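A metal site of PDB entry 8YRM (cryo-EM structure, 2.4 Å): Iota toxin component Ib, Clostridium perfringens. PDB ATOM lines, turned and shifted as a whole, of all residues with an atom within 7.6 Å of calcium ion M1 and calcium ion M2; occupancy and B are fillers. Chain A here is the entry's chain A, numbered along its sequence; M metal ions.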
ATOM      1  N   LEU A   3     -30.128   8.283  -4.173  1.00  0.00           N
ATOM      2  CA  LEU A   3     -28.837   8.661  -3.636  1.00  0.00           C
ATOM      3  C   LEU A   3     -28.265   9.758  -4.528  1.00  0.00           C
ATOM      4  O   LEU A   3     -28.087   9.535  -5.723  1.00  0.00           O
ATOM      5  CB  LEU A   3     -27.915   7.442  -3.567  1.00  0.00           C
ATOM      6  CG  LEU A   3     -26.470   7.726  -3.159  1.00  0.00           C
ATOM      7  CD1 LEU A   3     -26.422   8.370  -1.777  1.00  0.00           C
ATOM      8  CD2 LEU A   3     -25.658   6.441  -3.185  1.00  0.00           C
ATOM      9  N   ASP A   4     -28.004  10.913  -3.938  1.00  0.00           N
ATOM     10  CA  ASP A   4     -27.572  12.087  -4.676  1.00  0.00           C
ATOM     11  C   ASP A   4     -26.249  12.565  -4.084  1.00  0.00           C
ATOM     12  O   ASP A   4     -26.226  13.471  -3.245  1.00  0.00           O
ATOM     13  CB  ASP A   4     -28.655  13.146  -4.643  1.00  0.00           C
ATOM     14  CG  ASP A   4     -28.495  14.280  -5.643  1.00  0.00           C
ATOM     15  OD1 ASP A   4     -27.634  14.147  -6.525  1.00  0.00           O
ATOM     16  OD2 ASP A   4     -29.236  15.279  -5.516  1.00  0.00           O
ATOM     17  N   THR A   5     -25.152  11.969  -4.549  1.00  0.00           N
ATOM     18  CA  THR A   5     -23.850  12.239  -3.974  1.00  0.00           C
ATOM     19  C   THR A   5     -23.459  13.707  -4.141  1.00  0.00           C
ATOM     20  O   THR A   5     -22.871  14.283  -3.230  1.00  0.00           O
ATOM     21  CB  THR A   5     -22.803  11.339  -4.627  1.00  0.00           C
ATOM     22  OG1 THR A   5     -23.294  10.020  -4.449  1.00  0.00           O
ATOM     23  CG2 THR A   5     -21.432  11.525  -3.994  1.00  0.00           C
ATOM     24  N   ASP A   6     -23.773  14.306  -5.292  1.00  0.00           N
ATOM     25  CA  ASP A   6     -23.372  15.674  -5.585  1.00  0.00           C
ATOM     26  C   ASP A   6     -24.450  16.665  -5.161  1.00  0.00           C
ATOM     27  O   ASP A   6     -24.224  17.874  -5.259  1.00  0.00           O
ATOM     28  CB  ASP A   6     -23.019  15.836  -7.055  1.00  0.00           C
ATOM     29  CG  ASP A   6     -24.066  15.364  -8.047  1.00  0.00           C
ATOM     30  OD1 ASP A   6     -25.094  14.809  -7.601  1.00  0.00           O
ATOM     31  OD2 ASP A   6     -23.838  15.520  -9.241  1.00  0.00           O
ATOM     32  N   ASN A   7     -25.603  16.162  -4.716  1.00  0.00           N
ATOM     33  CA  ASN A   7     -26.687  16.984  -4.202  1.00  0.00           C
ATOM     34  C   ASN A   7     -27.175  17.957  -5.274  1.00  0.00           C
ATOM     35  O   ASN A   7     -27.297  19.154  -5.019  1.00  0.00           O
ATOM     36  CB  ASN A   7     -26.288  17.744  -2.946  1.00  0.00           C
ATOM     37  CG  ASN A   7     -25.749  16.822  -1.878  1.00  0.00           C
ATOM     38  OD1 ASN A   7     -26.445  15.894  -1.454  1.00  0.00           O
ATOM     39  ND2 ASN A   7     -24.514  17.058  -1.448  1.00  0.00           N
ATOM     40  N   ASP A   8     -27.479  17.447  -6.473  1.00  0.00           N
ATOM     41  CA  ASP A   8     -27.956  18.286  -7.555  1.00  0.00           C
ATOM     42  C   ASP A   8     -29.365  17.887  -7.984  1.00  0.00           C
ATOM     43  O   ASP A   8     -29.779  18.215  -9.081  1.00  0.00           O
ATOM     44  CB  ASP A   8     -27.006  18.248  -8.741  1.00  0.00           C
ATOM     45  CG  ASP A   8     -26.919  16.926  -9.481  1.00  0.00           C
ATOM     46  OD1 ASP A   8     -27.297  15.879  -8.897  1.00  0.00           O
ATOM     47  OD2 ASP A   8     -26.458  16.936 -10.630  1.00  0.00           O
ATOM     48  N   ASN A   9     -30.096  17.165  -7.120  1.00  0.00           N
ATOM     49  CA  ASN A   9     -31.480  16.787  -7.351  1.00  0.00           C
ATOM     50  C   ASN A   9     -31.631  15.734  -8.444  1.00  0.00           C
ATOM     51  O   ASN A   9     -32.750  15.504  -8.897  1.00  0.00           O
ATOM     52  CB  ASN A   9     -32.390  17.963  -7.700  1.00  0.00           C
ATOM     53  CG  ASN A   9     -32.395  19.012  -6.612  1.00  0.00           C
ATOM     54  OD1 ASN A   9     -32.327  18.680  -5.427  1.00  0.00           O
ATOM     55  ND2 ASN A   9     -32.457  20.281  -7.004  1.00  0.00           N
ATOM     56  N   ILE A  10     -30.543  15.067  -8.843  1.00  0.00           N
ATOM     57  CA  ILE A  10     -30.656  13.937  -9.756  1.00  0.00           C
ATOM     58  C   ILE A  10     -29.933  12.756  -9.125  1.00  0.00           C
ATOM     59  O   ILE A  10     -28.739  12.845  -8.847  1.00  0.00           O
ATOM     60  CB  ILE A  10     -30.065  14.251 -11.139  1.00  0.00           C
ATOM     61  CG1 ILE A  10     -30.480  15.633 -11.621  1.00  0.00           C
ATOM     62  CG2 ILE A  10     -30.431  13.169 -12.159  1.00  0.00           C
ATOM     63  CD1 ILE A  10     -29.650  16.115 -12.793  1.00  0.00           C
ATOM     64  N   PRO A  11     -30.635  11.627  -8.854  1.00  0.00           N
ATOM     65  CA  PRO A  11     -29.985  10.455  -8.253  1.00  0.00           C
ATOM     66  C   PRO A  11     -28.809   9.965  -9.084  1.00  0.00           C
ATOM     67  O   PRO A  11     -28.798  10.124 -10.307  1.00  0.00           O
ATOM     68  CB  PRO A  11     -31.118   9.421  -8.209  1.00  0.00           C
ATOM     69  CG  PRO A  11     -32.367  10.246  -8.182  1.00  0.00           C
ATOM     70  CD  PRO A  11     -32.077  11.435  -9.066  1.00  0.00           C
ATOM     71  N   ASP A  12     -27.856   9.314  -8.412  1.00  0.00           N
ATOM     72  CA  ASP A  12     -26.657   8.811  -9.051  1.00  0.00           C
ATOM     73  C   ASP A  12     -27.007   7.791 -10.123  1.00  0.00           C
ATOM     74  O   ASP A  12     -26.416   7.813 -11.208  1.00  0.00           O
ATOM     75  CB  ASP A  12     -25.716   8.192  -8.020  1.00  0.00           C
ATOM     76  CG  ASP A  12     -25.211   9.171  -6.980  1.00  0.00           C
ATOM     77  OD1 ASP A  12     -25.553  10.380  -7.089  1.00  0.00           O
ATOM     78  OD2 ASP A  12     -24.497   8.716  -6.055  1.00  0.00           O
ATOM     79  N   ALA A  13     -27.960   6.909  -9.829  1.00  0.00           N
ATOM     80  CA  ALA A  13     -28.341   5.880 -10.781  1.00  0.00           C
ATOM     81  C   ALA A  13     -28.880   6.532 -12.044  1.00  0.00           C
ATOM     82  O   ALA A  13     -28.616   6.060 -13.153  1.00  0.00           O
ATOM     83  CB  ALA A  13     -29.338   4.943 -10.153  1.00  0.00           C
ATOM     84  N   GLU A  15     -28.180   9.561 -13.198  1.00  0.00           N
ATOM     85  CA  GLU A  15     -27.128  10.225 -13.948  1.00  0.00           C
ATOM     86  C   GLU A  15     -26.258   9.222 -14.704  1.00  0.00           C
ATOM     87  O   GLU A  15     -25.892   9.488 -15.852  1.00  0.00           O
ATOM     88  CB  GLU A  15     -26.253  11.098 -13.051  1.00  0.00           C
ATOM     89  CG  GLU A  15     -27.032  12.192 -12.325  1.00  0.00           C
ATOM     90  CD  GLU A  15     -26.205  13.390 -11.931  1.00  0.00           C
ATOM     91  OE1 GLU A  15     -25.664  14.052 -12.841  1.00  0.00           O
ATOM     92  OE2 GLU A  15     -26.109  13.709 -10.739  1.00  0.00           O
ATOM     93  N   TYR A  19     -31.675   9.791 -17.924  1.00  0.00           N
ATOM     94  CA  TYR A  19     -32.828  10.348 -17.238  1.00  0.00           C
ATOM     95  C   TYR A  19     -33.441  11.470 -18.078  1.00  0.00           C
ATOM     96  O   TYR A  19     -32.833  11.958 -19.018  1.00  0.00           O
ATOM     97  CB  TYR A  19     -32.430  10.856 -15.864  1.00  0.00           C
ATOM     98  CG  TYR A  19     -31.494  12.044 -15.900  1.00  0.00           C
ATOM     99  CD1 TYR A  19     -30.114  11.881 -15.980  1.00  0.00           C
ATOM    100  CD2 TYR A  19     -31.990  13.344 -15.868  1.00  0.00           C
ATOM    101  CE1 TYR A  19     -29.253  12.954 -16.018  1.00  0.00           C
ATOM    102  CE2 TYR A  19     -31.136  14.443 -15.916  1.00  0.00           C
ATOM    103  CZ  TYR A  19     -29.761  14.240 -15.996  1.00  0.00           C
ATOM    104  OH  TYR A  19     -28.881  15.285 -16.018  1.00  0.00           O
ATOM    105  N   VAL A  42     -27.518  12.354 -19.723  1.00  0.00           N
ATOM    106  CA  VAL A  42     -26.570  11.714 -18.833  1.00  0.00           C
ATOM    107  C   VAL A  42     -25.641  12.793 -18.293  1.00  0.00           C
ATOM    108  O   VAL A  42     -25.454  13.827 -18.921  1.00  0.00           O
ATOM    109  CB  VAL A  42     -25.763  10.605 -19.540  1.00  0.00           C
ATOM    110  CG1 VAL A  42     -26.624   9.377 -19.804  1.00  0.00           C
ATOM    111  CG2 VAL A  42     -25.131  11.092 -20.825  1.00  0.00           C
ATOM    112  N   SER A  43     -25.075  12.555 -17.110  1.00  0.00           N
ATOM    113  CA  SER A  43     -24.185  13.521 -16.491  1.00  0.00           C
ATOM    114  C   SER A  43     -23.362  12.824 -15.422  1.00  0.00           C
ATOM    115  O   SER A  43     -23.571  11.644 -15.137  1.00  0.00           O
ATOM    116  CB  SER A  43     -24.931  14.715 -15.932  1.00  0.00           C
ATOM    117  OG  SER A  43     -26.187  14.343 -15.380  1.00  0.00           O
ATOM    118  N   SER A  44     -22.392  13.539 -14.861  1.00  0.00           N
ATOM    119  CA  SER A  44     -21.563  12.985 -13.808  1.00  0.00           C
ATOM    120  C   SER A  44     -22.317  13.013 -12.481  1.00  0.00           C
ATOM    121  O   SER A  44     -22.829  14.055 -12.073  1.00  0.00           O
ATOM    122  CB  SER A  44     -20.277  13.748 -13.689  1.00  0.00           C
ATOM    123  OG  SER A  44     -19.646  13.438 -12.453  1.00  0.00           O
ATOM    124  N   TYR A  45     -22.334  11.878 -11.787  1.00  0.00           N
ATOM    125  CA  TYR A  45     -22.989  11.808 -10.497  1.00  0.00           C
ATOM    126  C   TYR A  45     -22.080  12.347  -9.395  1.00  0.00           C
ATOM    127  O   TYR A  45     -22.527  12.476  -8.263  1.00  0.00           O
ATOM    128  CB  TYR A  45     -23.446  10.384 -10.208  1.00  0.00           C
ATOM    129  CG  TYR A  45     -22.336   9.409  -9.880  1.00  0.00           C
ATOM    130  CD1 TYR A  45     -21.705   8.692 -10.886  1.00  0.00           C
ATOM    131  CD2 TYR A  45     -21.914   9.212  -8.572  1.00  0.00           C
ATOM    132  CE1 TYR A  45     -20.693   7.792 -10.596  1.00  0.00           C
ATOM    133  CE2 TYR A  45     -20.897   8.316  -8.274  1.00  0.00           C
ATOM    134  CZ  TYR A  45     -20.291   7.603  -9.295  1.00  0.00           C
ATOM    135  OH  TYR A  45     -19.294   6.715  -9.004  1.00  0.00           O
ATOM    136  N   LEU A  46     -20.827  12.702  -9.728  1.00  0.00           N
ATOM    137  CA  LEU A  46     -19.896  13.292  -8.775  1.00  0.00           C
ATOM    138  C   LEU A  46     -19.715  14.791  -9.000  1.00  0.00           C
ATOM    139  O   LEU A  46     -19.030  15.448  -8.230  1.00  0.00           O
ATOM    140  CB  LEU A  46     -18.561  12.567  -8.824  1.00  0.00           C
ATOM    141  CG  LEU A  46     -18.522  11.168  -8.206  1.00  0.00           C
ATOM    142  CD1 LEU A  46     -17.089  10.663  -8.196  1.00  0.00           C
ATOM    143  CD2 LEU A  46     -19.111  11.104  -6.804  1.00  0.00           C
ATOM    144  N   GLU A  47     -20.328  15.348 -10.053  1.00  0.00           N
ATOM    145  CA  GLU A  47     -20.222  16.770 -10.324  1.00  0.00           C
ATOM    146  C   GLU A  47     -21.620  17.372 -10.451  1.00  0.00           C
ATOM    147  O   GLU A  47     -22.463  16.847 -11.173  1.00  0.00           O
ATOM    148  CB  GLU A  47     -19.450  16.995 -11.618  1.00  0.00           C
ATOM    149  CG  GLU A  47     -17.943  17.072 -11.404  1.00  0.00           C
ATOM    150  CD  GLU A  47     -17.499  18.310 -10.640  1.00  0.00           C
ATOM    151  OE1 GLU A  47     -18.274  19.311 -10.608  1.00  0.00           O
ATOM    152  OE2 GLU A  47     -16.399  18.264 -10.059  1.00  0.00           O
ATOM    153  N   SER A  48     -21.850  18.477  -9.748  1.00  0.00           N
ATOM    154  CA  SER A  48     -23.113  19.172  -9.868  1.00  0.00           C
ATOM    155  C   SER A  48     -23.187  19.930 -11.197  1.00  0.00           C
ATOM    156  O   SER A  48     -24.253  20.087 -11.778  1.00  0.00           O
ATOM    157  CB  SER A  48     -23.333  20.091  -8.703  1.00  0.00           C
ATOM    158  OG  SER A  48     -22.427  21.175  -8.746  1.00  0.00           O
ATOM    159  N   ASN A  49     -22.034  20.419 -11.659  1.00  0.00           N
ATOM    160  CA  ASN A  49     -21.932  21.148 -12.902  1.00  0.00           C
ATOM    161  C   ASN A  49     -20.993  20.412 -13.844  1.00  0.00           C
ATOM    162  O   ASN A  49     -19.834  20.777 -13.961  1.00  0.00           O
ATOM    163  CB  ASN A  49     -21.427  22.557 -12.651  1.00  0.00           C
ATOM    164  CG  ASN A  49     -22.354  23.348 -11.756  1.00  0.00           C
ATOM    165  OD1 ASN A  49     -22.765  22.855 -10.703  1.00  0.00           O
ATOM    166  ND2 ASN A  49     -22.688  24.573 -12.136  1.00  0.00           N
ATOM    167  N   THR A  50     -21.503  19.393 -14.539  1.00  0.00           N
ATOM    168  CA  THR A  50     -20.679  18.520 -15.352  1.00  0.00           C
ATOM    169  C   THR A  50     -19.924  19.305 -16.434  1.00  0.00           C
ATOM    170  O   THR A  50     -18.771  18.987 -16.701  1.00  0.00           O
ATOM    171  CB  THR A  50     -21.546  17.436 -15.971  1.00  0.00           C
ATOM    172  OG1 THR A  50     -22.110  16.719 -14.885  1.00  0.00           O
ATOM    173  CG2 THR A  50     -20.730  16.516 -16.879  1.00  0.00           C
ATOM    174  N   THR A  56     -26.216  24.079 -12.845  1.00  0.00           N
ATOM    175  CA  THR A  56     -26.077  22.682 -12.475  1.00  0.00           C
ATOM    176  C   THR A  56     -26.720  21.787 -13.526  1.00  0.00           C
ATOM    177  O   THR A  56     -27.439  22.264 -14.410  1.00  0.00           O
ATOM    178  CB  THR A  56     -26.678  22.422 -11.089  1.00  0.00           C
ATOM    179  OG1 THR A  56     -28.098  22.411 -11.209  1.00  0.00           O
ATOM    180  CG2 THR A  56     -26.249  23.452 -10.063  1.00  0.00           C
ATOM    181  N   ASP A  57     -26.481  20.492 -13.408  1.00  0.00           N
ATOM    182  CA  ASP A  57     -27.059  19.495 -14.303  1.00  0.00           C
ATOM    183  C   ASP A  57     -28.586  19.554 -14.269  1.00  0.00           C
ATOM    184  O   ASP A  57     -29.226  19.409 -15.303  1.00  0.00           O
ATOM    185  CB  ASP A  57     -26.560  18.110 -13.948  1.00  0.00           C
ATOM    186  CG  ASP A  57     -25.040  17.947 -14.023  1.00  0.00           C
ATOM    187  OD1 ASP A  57     -24.375  18.823 -14.601  1.00  0.00           O
ATOM    188  OD2 ASP A  57     -24.536  16.958 -13.493  1.00  0.00           O
ATOM    189  N   TYR A  58     -29.175  19.736 -13.081  1.00  0.00           N
ATOM    190  CA  TYR A  58     -30.624  19.768 -12.949  1.00  0.00           C
ATOM    191  C   TYR A  58     -31.174  21.057 -13.561  1.00  0.00           C
ATOM    192  O   TYR A  58     -32.172  21.024 -14.275  1.00  0.00           O
ATOM    193  CB  TYR A  58     -31.062  19.611 -11.488  1.00  0.00           C
ATOM    194  CG  TYR A  58     -32.547  19.855 -11.325  1.00  0.00           C
ATOM    195  CD1 TYR A  58     -33.466  18.860 -11.655  1.00  0.00           C
ATOM    196  CD2 TYR A  58     -33.042  21.090 -10.938  1.00  0.00           C
ATOM    197  CE1 TYR A  58     -34.827  19.081 -11.578  1.00  0.00           C
ATOM    198  CE2 TYR A  58     -34.408  21.321 -10.852  1.00  0.00           C
ATOM    199  CZ  TYR A  58     -35.302  20.322 -11.168  1.00  0.00           C
ATOM    200  OH  TYR A  58     -36.644  20.532 -11.071  1.00  0.00           O
ATOM    201  N   PRO A  76     -26.778  18.577 -20.208  1.00  0.00           N
ATOM    202  CA  PRO A  76     -25.691  18.723 -19.239  1.00  0.00           C
ATOM    203  C   PRO A  76     -24.283  18.637 -19.829  1.00  0.00           C
ATOM    204  O   PRO A  76     -23.360  19.207 -19.268  1.00  0.00           O
ATOM    205  CB  PRO A  76     -25.959  17.626 -18.229  1.00  0.00           C
ATOM    206  CG  PRO A  76     -27.453  17.433 -18.327  1.00  0.00           C
ATOM    207  CD  PRO A  76     -27.751  17.568 -19.801  1.00  0.00           C
HETATM  208 CA    CA M   1     -24.337  15.698 -11.462  1.00  0.00          CA
HETATM  209 CA    CA M   2     -26.665  13.874  -8.560  1.00  0.00          CA
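OG of Ser 44 sits at hydrogen-bond distance from N of Leu 46 (3.1 Å). The side-chain carboxylate (OD1) of Asp 12 lies within hydrogen-bond range of the backbone NH (N) of Thr 5 (3.0 Å). OD2 of Asp 4 lies within hydrogen-bond range of N of Asn 9 (2.6 Å). The backbone carbonyl oxygen (O) of Asp 4 sits close to the side-chain amide oxygen (OD1) of Asn 7, 3.0 Å away. The backbone NH (N) of Asp 57 sits at hydrogen-bond distance from the backbone carbonyl oxygen (O) of Ser 48 (2.8 Å). N of Asp 12 lies within hydrogen-bond range of O of Leu 3 (2.7 Å). The backbone NH (N) of Ser 44 sits at hydrogen-bond distance from the side-chain hydroxyl (OG1) of Thr 50, at 3.2 Å. The backbone carbonyl oxygen (O) of Glu 15 is in hydrogen-bond range of the backbone NH (N) of Ser 43, 3.4 Å away.
Six residues have an atom within 4 Å of calcium ion M1: Asp 6, Asp 8, Glu 15, Ser 44, Glu 47 and Asp 57. The nearest printed residue that does not touch calcium ion M1 is Ser 48 (4.01 Å).
Calcium ion M1 is bound by the backbone carbonyl oxygen (O) of Glu 47 (2.2 Å). The side-chain carboxylate (OD2) of Asp 6 binds calcium ion M1 (2.3 Å). O of Ser 44 is bound to calcium ion M1 (2.3 Å). OD2 of Asp 57 is bound to calcium ion M1 (2.4 Å). The side-chain carboxylate (OE1) of Glu 15 binds calcium ion M1. Calcium ion M1 is bound by OD2 of Asp 8 (2.6 Å). Calcium ion M1 is bound by OE2 of Glu 15 (2.8 Å). Calcium ion M1 has seven donor atoms within binding distance.
Asp 12 touches calcium ion M2. The nearest printed residue that does not touch calcium ion M2 is Tyr 45 (4.4 Å).
Calcium ion M2 is bound by OD1 of Asp 6 (2.1 Å), OD1 of Asp 8 (2.1 Å), OE2 of Glu 15 (2.3 Å), OD1 of Asp 4 (2.3 Å) and O of Ile 10 (2.3 Å).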
